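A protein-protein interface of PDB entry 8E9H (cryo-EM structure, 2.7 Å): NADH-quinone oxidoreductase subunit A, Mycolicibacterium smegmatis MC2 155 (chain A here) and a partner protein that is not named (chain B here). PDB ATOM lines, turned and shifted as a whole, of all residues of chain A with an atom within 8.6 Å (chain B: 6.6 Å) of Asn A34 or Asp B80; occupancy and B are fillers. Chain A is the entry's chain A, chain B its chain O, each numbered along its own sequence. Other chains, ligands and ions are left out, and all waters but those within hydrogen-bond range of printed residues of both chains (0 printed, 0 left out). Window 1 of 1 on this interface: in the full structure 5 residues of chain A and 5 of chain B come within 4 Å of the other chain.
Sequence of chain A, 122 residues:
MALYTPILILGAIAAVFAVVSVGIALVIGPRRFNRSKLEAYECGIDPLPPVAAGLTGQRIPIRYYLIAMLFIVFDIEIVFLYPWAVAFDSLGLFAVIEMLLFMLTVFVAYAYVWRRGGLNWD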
ATOM      1  N   ARG A  31       3.177  22.965  -7.485  1.00  0.00           N
ATOM      2  CA  ARG A  31       4.021  22.062  -8.248  1.00  0.00           C
ATOM      3  C   ARG A  31       4.617  21.040  -7.299  1.00  0.00           C
ATOM      4  O   ARG A  31       5.160  21.396  -6.251  1.00  0.00           O
ATOM      5  CB  ARG A  31       5.133  22.807  -8.985  1.00  0.00           C
ATOM      6  CG  ARG A  31       4.638  23.953  -9.837  1.00  0.00           C
ATOM      7  CD  ARG A  31       5.620  24.273 -10.941  1.00  0.00           C
ATOM      8  NE  ARG A  31       5.361  23.457 -12.122  1.00  0.00           N
ATOM      9  CZ  ARG A  31       6.235  22.637 -12.692  1.00  0.00           C
ATOM     10  NH1 ARG A  31       7.464  22.492 -12.221  1.00  0.00           N
ATOM     11  NH2 ARG A  31       5.865  21.940 -13.761  1.00  0.00           N
ATOM     12  N   ARG A  32       4.513  19.768  -7.673  1.00  0.00           N
ATOM     13  CA  ARG A  32       4.965  18.684  -6.808  1.00  0.00           C
ATOM     14  C   ARG A  32       5.558  17.607  -7.710  1.00  0.00           C
ATOM     15  O   ARG A  32       4.821  16.908  -8.409  1.00  0.00           O
ATOM     16  CB  ARG A  32       3.818  18.141  -5.969  1.00  0.00           C
ATOM     17  CG  ARG A  32       4.194  16.988  -5.062  1.00  0.00           C
ATOM     18  CD  ARG A  32       5.067  17.455  -3.918  1.00  0.00           C
ATOM     19  NE  ARG A  32       5.607  16.338  -3.155  1.00  0.00           N
ATOM     20  CZ  ARG A  32       6.364  16.466  -2.076  1.00  0.00           C
ATOM     21  NH1 ARG A  32       6.691  17.655  -1.597  1.00  0.00           N
ATOM     22  NH2 ARG A  32       6.812  15.373  -1.465  1.00  0.00           N
ATOM     23  N   PHE A  33       6.881  17.485  -7.695  1.00  0.00           N
ATOM     24  CA  PHE A  33       7.524  16.466  -8.507  1.00  0.00           C
ATOM     25  C   PHE A  33       7.055  15.085  -8.082  1.00  0.00           C
ATOM     26  O   PHE A  33       7.000  14.772  -6.890  1.00  0.00           O
ATOM     27  CB  PHE A  33       9.041  16.561  -8.390  1.00  0.00           C
ATOM     28  CG  PHE A  33       9.758  15.442  -9.075  1.00  0.00           C
ATOM     29  CD1 PHE A  33      10.127  14.308  -8.377  1.00  0.00           C
ATOM     30  CD2 PHE A  33      10.040  15.509 -10.425  1.00  0.00           C
ATOM     31  CE1 PHE A  33      10.777  13.272  -9.009  1.00  0.00           C
ATOM     32  CE2 PHE A  33      10.691  14.477 -11.061  1.00  0.00           C
ATOM     33  CZ  PHE A  33      11.059  13.357 -10.352  1.00  0.00           C
ATOM     34  N   ASN A  34       6.718  14.258  -9.064  1.00  0.00           N
ATOM     35  CA  ASN A  34       6.276  12.893  -8.799  1.00  0.00           C
ATOM     36  C   ASN A  34       6.519  12.079 -10.055  1.00  0.00           C
ATOM     37  O   ASN A  34       5.954  12.387 -11.107  1.00  0.00           O
ATOM     38  CB  ASN A  34       4.805  12.863  -8.404  1.00  0.00           C
ATOM     39  CG  ASN A  34       4.282  11.457  -8.211  1.00  0.00           C
ATOM     40  OD1 ASN A  34       4.439  10.599  -9.076  1.00  0.00           O
ATOM     41  ND2 ASN A  34       3.652  11.214  -7.071  1.00  0.00           N
ATOM     42  N   ARG A  35       7.343  11.039  -9.948  1.00  0.00           N
ATOM     43  CA  ARG A  35       7.702  10.265 -11.129  1.00  0.00           C
ATOM     44  C   ARG A  35       6.465   9.683 -11.795  1.00  0.00           C
ATOM     45  O   ARG A  35       6.341   9.701 -13.024  1.00  0.00           O
ATOM     46  CB  ARG A  35       8.679   9.159 -10.744  1.00  0.00           C
ATOM     47  CG  ARG A  35      10.037   9.684 -10.352  1.00  0.00           C
ATOM     48  CD  ARG A  35      10.963   8.576  -9.916  1.00  0.00           C
ATOM     49  NE  ARG A  35      12.311   9.079  -9.698  1.00  0.00           N
ATOM     50  CZ  ARG A  35      12.680   9.794  -8.644  1.00  0.00           C
ATOM     51  NH1 ARG A  35      11.825  10.098  -7.682  1.00  0.00           N
ATOM     52  NH2 ARG A  35      13.938  10.217  -8.555  1.00  0.00           N
ATOM     53  N   SER A  36       5.534   9.158 -10.998  1.00  0.00           N
ATOM     54  CA  SER A  36       4.304   8.623 -11.569  1.00  0.00           C
ATOM     55  C   SER A  36       3.489   9.712 -12.249  1.00  0.00           C
ATOM     56  O   SER A  36       2.871   9.462 -13.288  1.00  0.00           O
ATOM     57  CB  SER A  36       3.475   7.942 -10.486  1.00  0.00           C
ATOM     58  OG  SER A  36       4.217   6.913  -9.858  1.00  0.00           O
ATOM     59  N   LYS A  37       3.471  10.917 -11.684  1.00  0.00           N
ATOM     60  CA  LYS A  37       2.738  12.008 -12.312  1.00  0.00           C
ATOM     61  C   LYS A  37       3.326  12.348 -13.674  1.00  0.00           C
ATOM     62  O   LYS A  37       2.590  12.569 -14.641  1.00  0.00           O
ATOM     63  CB  LYS A  37       2.752  13.236 -11.404  1.00  0.00           C
ATOM     64  CG  LYS A  37       1.931  14.399 -11.925  1.00  0.00           C
ATOM     65  CD  LYS A  37       2.130  15.645 -11.087  1.00  0.00           C
ATOM     66  CE  LYS A  37       1.471  15.516  -9.730  1.00  0.00           C
ATOM     67  NZ  LYS A  37       1.854  16.629  -8.824  1.00  0.00           N
ATOM     68  N   LEU A  38       4.653  12.390 -13.770  1.00  0.00           N
ATOM     69  CA  LEU A  38       5.289  12.879 -14.985  1.00  0.00           C
ATOM     70  C   LEU A  38       5.270  11.856 -16.111  1.00  0.00           C
ATOM     71  O   LEU A  38       5.280  12.241 -17.284  1.00  0.00           O
ATOM     72  CB  LEU A  38       6.726  13.294 -14.686  1.00  0.00           C
ATOM     73  CG  LEU A  38       6.886  14.353 -13.596  1.00  0.00           C
ATOM     74  CD1 LEU A  38       8.322  14.830 -13.542  1.00  0.00           C
ATOM     75  CD2 LEU A  38       5.944  15.517 -13.821  1.00  0.00           C
ATOM     76  N   GLU A  39       5.251  10.567 -15.795  1.00  0.00           N
ATOM     77  CA  GLU A  39       5.324   9.570 -16.848  1.00  0.00           C
ATOM     78  C   GLU A  39       4.024   9.538 -17.646  1.00  0.00           C
ATOM     79  O   GLU A  39       2.982  10.035 -17.215  1.00  0.00           O
ATOM     80  CB  GLU A  39       5.631   8.193 -16.269  1.00  0.00           C
ATOM     81  CG  GLU A  39       4.526   7.598 -15.434  1.00  0.00           C
ATOM     82  CD  GLU A  39       4.984   6.374 -14.669  1.00  0.00           C
ATOM     83  OE1 GLU A  39       6.201   6.100 -14.661  1.00  0.00           O
ATOM     84  OE2 GLU A  39       4.129   5.686 -14.076  1.00  0.00           O
ATOM     85  N   ASP A  46       1.189   0.843 -15.931  1.00  0.00           N
ATOM     86  CA  ASP A  46       2.552   1.340 -15.991  1.00  0.00           C
ATOM     87  C   ASP A  46       2.967   1.533 -17.446  1.00  0.00           C
ATOM     88  O   ASP A  46       2.739   0.651 -18.278  1.00  0.00           O
ATOM     89  CB  ASP A  46       3.514   0.374 -15.306  1.00  0.00           C
ATOM     90  CG  ASP A  46       3.215   0.195 -13.834  1.00  0.00           C
ATOM     91  OD1 ASP A  46       2.274   0.846 -13.334  1.00  0.00           O
ATOM     92  OD2 ASP A  46       3.923  -0.594 -13.177  1.00  0.00           O
ATOM     93  N   ALA B  75       4.174   5.255   1.174  1.00  0.00           N
ATOM     94  CA  ALA B  75       5.442   4.681   0.738  1.00  0.00           C
ATOM     95  C   ALA B  75       5.619   4.850  -0.762  1.00  0.00           C
ATOM     96  O   ALA B  75       6.679   5.283  -1.237  1.00  0.00           O
ATOM     97  CB  ALA B  75       5.506   3.205   1.124  1.00  0.00           C
ATOM     98  N   LYS B  76       4.580   4.520  -1.525  1.00  0.00           N
ATOM     99  CA  LYS B  76       4.652   4.702  -2.969  1.00  0.00           C
ATOM    100  C   LYS B  76       4.886   6.166  -3.308  1.00  0.00           C
ATOM    101  O   LYS B  76       5.722   6.493  -4.159  1.00  0.00           O
ATOM    102  CB  LYS B  76       3.365   4.191  -3.615  1.00  0.00           C
ATOM    103  CG  LYS B  76       3.383   4.148  -5.127  1.00  0.00           C
ATOM    104  CD  LYS B  76       4.304   3.063  -5.639  1.00  0.00           C
ATOM    105  CE  LYS B  76       4.216   2.935  -7.144  1.00  0.00           C
ATOM    106  NZ  LYS B  76       4.906   4.057  -7.828  1.00  0.00           N
ATOM    107  N   GLN B  77       4.178   7.065  -2.625  1.00  0.00           N
ATOM    108  CA  GLN B  77       4.320   8.490  -2.894  1.00  0.00           C
ATOM    109  C   GLN B  77       5.739   8.964  -2.626  1.00  0.00           C
ATOM    110  O   GLN B  77       6.325   9.690  -3.433  1.00  0.00           O
ATOM    111  CB  GLN B  77       3.329   9.278  -2.041  1.00  0.00           C
ATOM    112  CG  GLN B  77       3.402  10.772  -2.247  1.00  0.00           C
ATOM    113  CD  GLN B  77       2.207  11.494  -1.676  1.00  0.00           C
ATOM    114  OE1 GLN B  77       1.171  10.887  -1.408  1.00  0.00           O
ATOM    115  NE2 GLN B  77       2.341  12.799  -1.487  1.00  0.00           N
ATOM    116  N   VAL B  78       6.312   8.567  -1.492  1.00  0.00           N
ATOM    117  CA  VAL B  78       7.634   9.068  -1.134  1.00  0.00           C
ATOM    118  C   VAL B  78       8.682   8.508  -2.079  1.00  0.00           C
ATOM    119  O   VAL B  78       9.623   9.210  -2.466  1.00  0.00           O
ATOM    120  CB  VAL B  78       7.965   8.749   0.335  1.00  0.00           C
ATOM    121  CG1 VAL B  78       6.968   9.425   1.259  1.00  0.00           C
ATOM    122  CG2 VAL B  78       7.997   7.258   0.574  1.00  0.00           C
ATOM    123  N   LYS B  79       8.542   7.243  -2.478  1.00  0.00           N
ATOM    124  CA  LYS B  79       9.518   6.699  -3.413  1.00  0.00           C
ATOM    125  C   LYS B  79       9.337   7.275  -4.809  1.00  0.00           C
ATOM    126  O   LYS B  79      10.264   7.214  -5.622  1.00  0.00           O
ATOM    127  CB  LYS B  79       9.437   5.177  -3.447  1.00  0.00           C
ATOM    128  CG  LYS B  79      10.173   4.525  -2.293  1.00  0.00           C
ATOM    129  CD  LYS B  79      10.414   3.052  -2.526  1.00  0.00           C
ATOM    130  CE  LYS B  79      11.274   2.463  -1.421  1.00  0.00           C
ATOM    131  NZ  LYS B  79      12.578   3.164  -1.287  1.00  0.00           N
ATOM    132  N   ASP B  80       8.165   7.835  -5.110  1.00  0.00           N
ATOM    133  CA  ASP B  80       7.980   8.493  -6.397  1.00  0.00           C
ATOM    134  C   ASP B  80       8.262   9.989  -6.355  1.00  0.00           C
ATOM    135  O   ASP B  80       8.309  10.618  -7.416  1.00  0.00           O
ATOM    136  CB  ASP B  80       6.556   8.274  -6.908  1.00  0.00           C
ATOM    137  CG  ASP B  80       6.348   6.887  -7.476  1.00  0.00           C
ATOM    138  OD1 ASP B  80       7.347   6.236  -7.846  1.00  0.00           O
ATOM    139  OD2 ASP B  80       5.182   6.451  -7.564  1.00  0.00           O
ATOM    140  N   GLU B  81       8.450  10.571  -5.175  1.00  0.00           N
ATOM    141  CA  GLU B  81       8.544  12.018  -5.047  1.00  0.00           C
ATOM    142  C   GLU B  81       9.840  12.516  -4.431  1.00  0.00           C
ATOM    143  O   GLU B  81      10.297  13.596  -4.804  1.00  0.00           O
ATOM    144  CB  GLU B  81       7.372  12.548  -4.212  1.00  0.00           C
ATOM    145  CG  GLU B  81       6.023  12.361  -4.877  1.00  0.00           C
ATOM    146  CD  GLU B  81       4.907  13.057  -4.133  1.00  0.00           C
ATOM    147  OE1 GLU B  81       5.119  13.431  -2.961  1.00  0.00           O
ATOM    148  OE2 GLU B  81       3.817  13.228  -4.716  1.00  0.00           O
ATOM    149  N   ILE B  82      10.441  11.778  -3.503  1.00  0.00           N
ATOM    150  CA  ILE B  82      11.667  12.199  -2.835  1.00  0.00           C
ATOM    151  C   ILE B  82      12.830  11.448  -3.457  1.00  0.00           C
ATOM    152  O   ILE B  82      12.845  10.212  -3.473  1.00  0.00           O
ATOM    153  CB  ILE B  82      11.604  11.959  -1.319  1.00  0.00           C
ATOM    154  CG1 ILE B  82      10.493  12.799  -0.688  1.00  0.00           C
ATOM    155  CG2 ILE B  82      12.941  12.282  -0.675  1.00  0.00           C
ATOM    156  CD1 ILE B  82       9.154  12.124  -0.657  1.00  0.00           C
ATOM    157  N   ASP B  83      13.802  12.194  -3.969  1.00  0.00           N
ATOM    158  CA  ASP B  83      15.013  11.585  -4.499  1.00  0.00           C
ATOM    159  C   ASP B  83      15.928  11.183  -3.353  1.00  0.00           C
ATOM    160  O   ASP B  83      16.110  11.939  -2.394  1.00  0.00           O
ATOM    161  CB  ASP B  83      15.730  12.555  -5.436  1.00  0.00           C
ATOM    162  N   CYS B  85      15.359   8.894  -1.156  1.00  0.00           N
ATOM    163  CA  CYS B  85      14.555   8.742   0.041  1.00  0.00           C
ATOM    164  C   CYS B  85      15.064   7.560   0.864  1.00  0.00           C
ATOM    165  O   CYS B  85      15.638   6.616   0.320  1.00  0.00           O
ATOM    166  CB  CYS B  85      13.089   8.528  -0.315  1.00  0.00           C
ATOM    167  SG  CYS B  85      12.742   6.938  -1.079  1.00  0.00           S
ATOM    168  N   ARG B 105       6.715  -1.001  -2.863  1.00  0.00           N
ATOM    169  CA  ARG B 105       8.165  -0.985  -3.002  1.00  0.00           C
ATOM    170  C   ARG B 105       8.858  -0.700  -1.680  1.00  0.00           C
ATOM    171  O   ARG B 105      10.039  -0.350  -1.657  1.00  0.00           O
ATOM    172  CB  ARG B 105       8.604   0.023  -4.065  1.00  0.00           C
ATOM    173  CG  ARG B 105       8.361  -0.468  -5.474  1.00  0.00           C
ATOM    174  CD  ARG B 105       8.161   0.674  -6.438  1.00  0.00           C
ATOM    175  NE  ARG B 105       8.056   0.202  -7.812  1.00  0.00           N
ATOM    176  CZ  ARG B 105       6.934  -0.214  -8.381  1.00  0.00           C
ATOM    177  NH1 ARG B 105       5.796  -0.270  -7.707  1.00  0.00           N
ATOM    178  NH2 ARG B 105       6.952  -0.587  -9.656  1.00  0.00           N
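N of Arg A35 lies within hydrogen-bond range of O of Asp B80 (2.7 Å). The side-chain hydroxyl of Ser A36 is in hydrogen-bond range of the side-chain carboxylate of Asp B80. The side-chain carboxylate (OE1) of Glu B81 lies within salt-bridge range of the guanidinium group (NE) of Arg A32, 3.0 Å away. The side-chain carboxylate (OE2) of Glu B81 lies within hydrogen-bond range of the side-chain amide nitrogen (ND2) of Asn A34, at 3.1 Å.
Asn A34 touches just these residues of chain B: Asp B80 (3.3 Å) and Glu B81 (3.1 Å). Printed residues of chain A within 4 Å of Asp B80: Phe A33 (3.96 Å), Asn A34 (3.3 Å), Arg A35 (2.7 Å) and Ser A36 (2.5 Å). Of the printed residues of chain B, Phe A33 touches Asp B80 (3.96 Å) and Glu B81 (3.3 Å). Printed residues of chain B within 4 Å of Arg A35: Lys B79 and Asp B80. Asp B83 touches none of the printed residues of chain A. Lys A37 touches none of the printed residues of chain B. The nearest residue of chain B that does not touch Asn A34 is Gln B77 (4.8 Å). The nearest residue of chain A that does not touch Asp B80 is Lys A37 (6.3 Å). The nearest printed residue of chain A that does not touch Lys B76 is Asn A34 (5.9 Å).
Hydrophobic or aromatic side chains of chain A within 4 Å of the printed part of chain B: Phe A33. Along chain A the printed residues that touch a printed residue of chain B span positions 32 to 36. Printed residues of chain B that touch a printed residue of chain A: Lys B76, Lys B79, Asp B80 and Glu B81. Among the printed residues, 9 pairs touch across the chains.
Among the printed residues, pairs that only touch across the chains: Phe A33 with Asp B80 (3.96 Å), Phe A33 with Glu B81 (3.3 Å), Asn A34 with Asp B80 (3.3 Å), Arg A35 with Lys B79 (3.9 Å) and Ser A36 with Lys B76 (3.6 Å).
The side-chain carboxylate (OD2) of Asp B80 is in salt-bridge range of the side-chain amino group (NZ) of Lys B76 (2.4 Å). NE2 of Gln B77 is in hydrogen-bond range of OE1 of Glu B81, 3.2 Å away. The side-chain sulfur (SG) of Cys B85 sits close to the side-chain amino group (NZ) of Lys B79, 3.8 Å away. The side-chain amino group of Lys A37 lies within hydrogen-bond range of the backbone carbonyl oxygen of Arg A32, at 3.0 Å. The side-chain amide oxygen (OD1) of Asn A34 is in hydrogen-bond range of the backbone NH (N) of Ser A36. The side-chain amide oxygen of Asn A34 is in hydrogen-bond range of the backbone NH of Lys A37 (2.8 Å).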
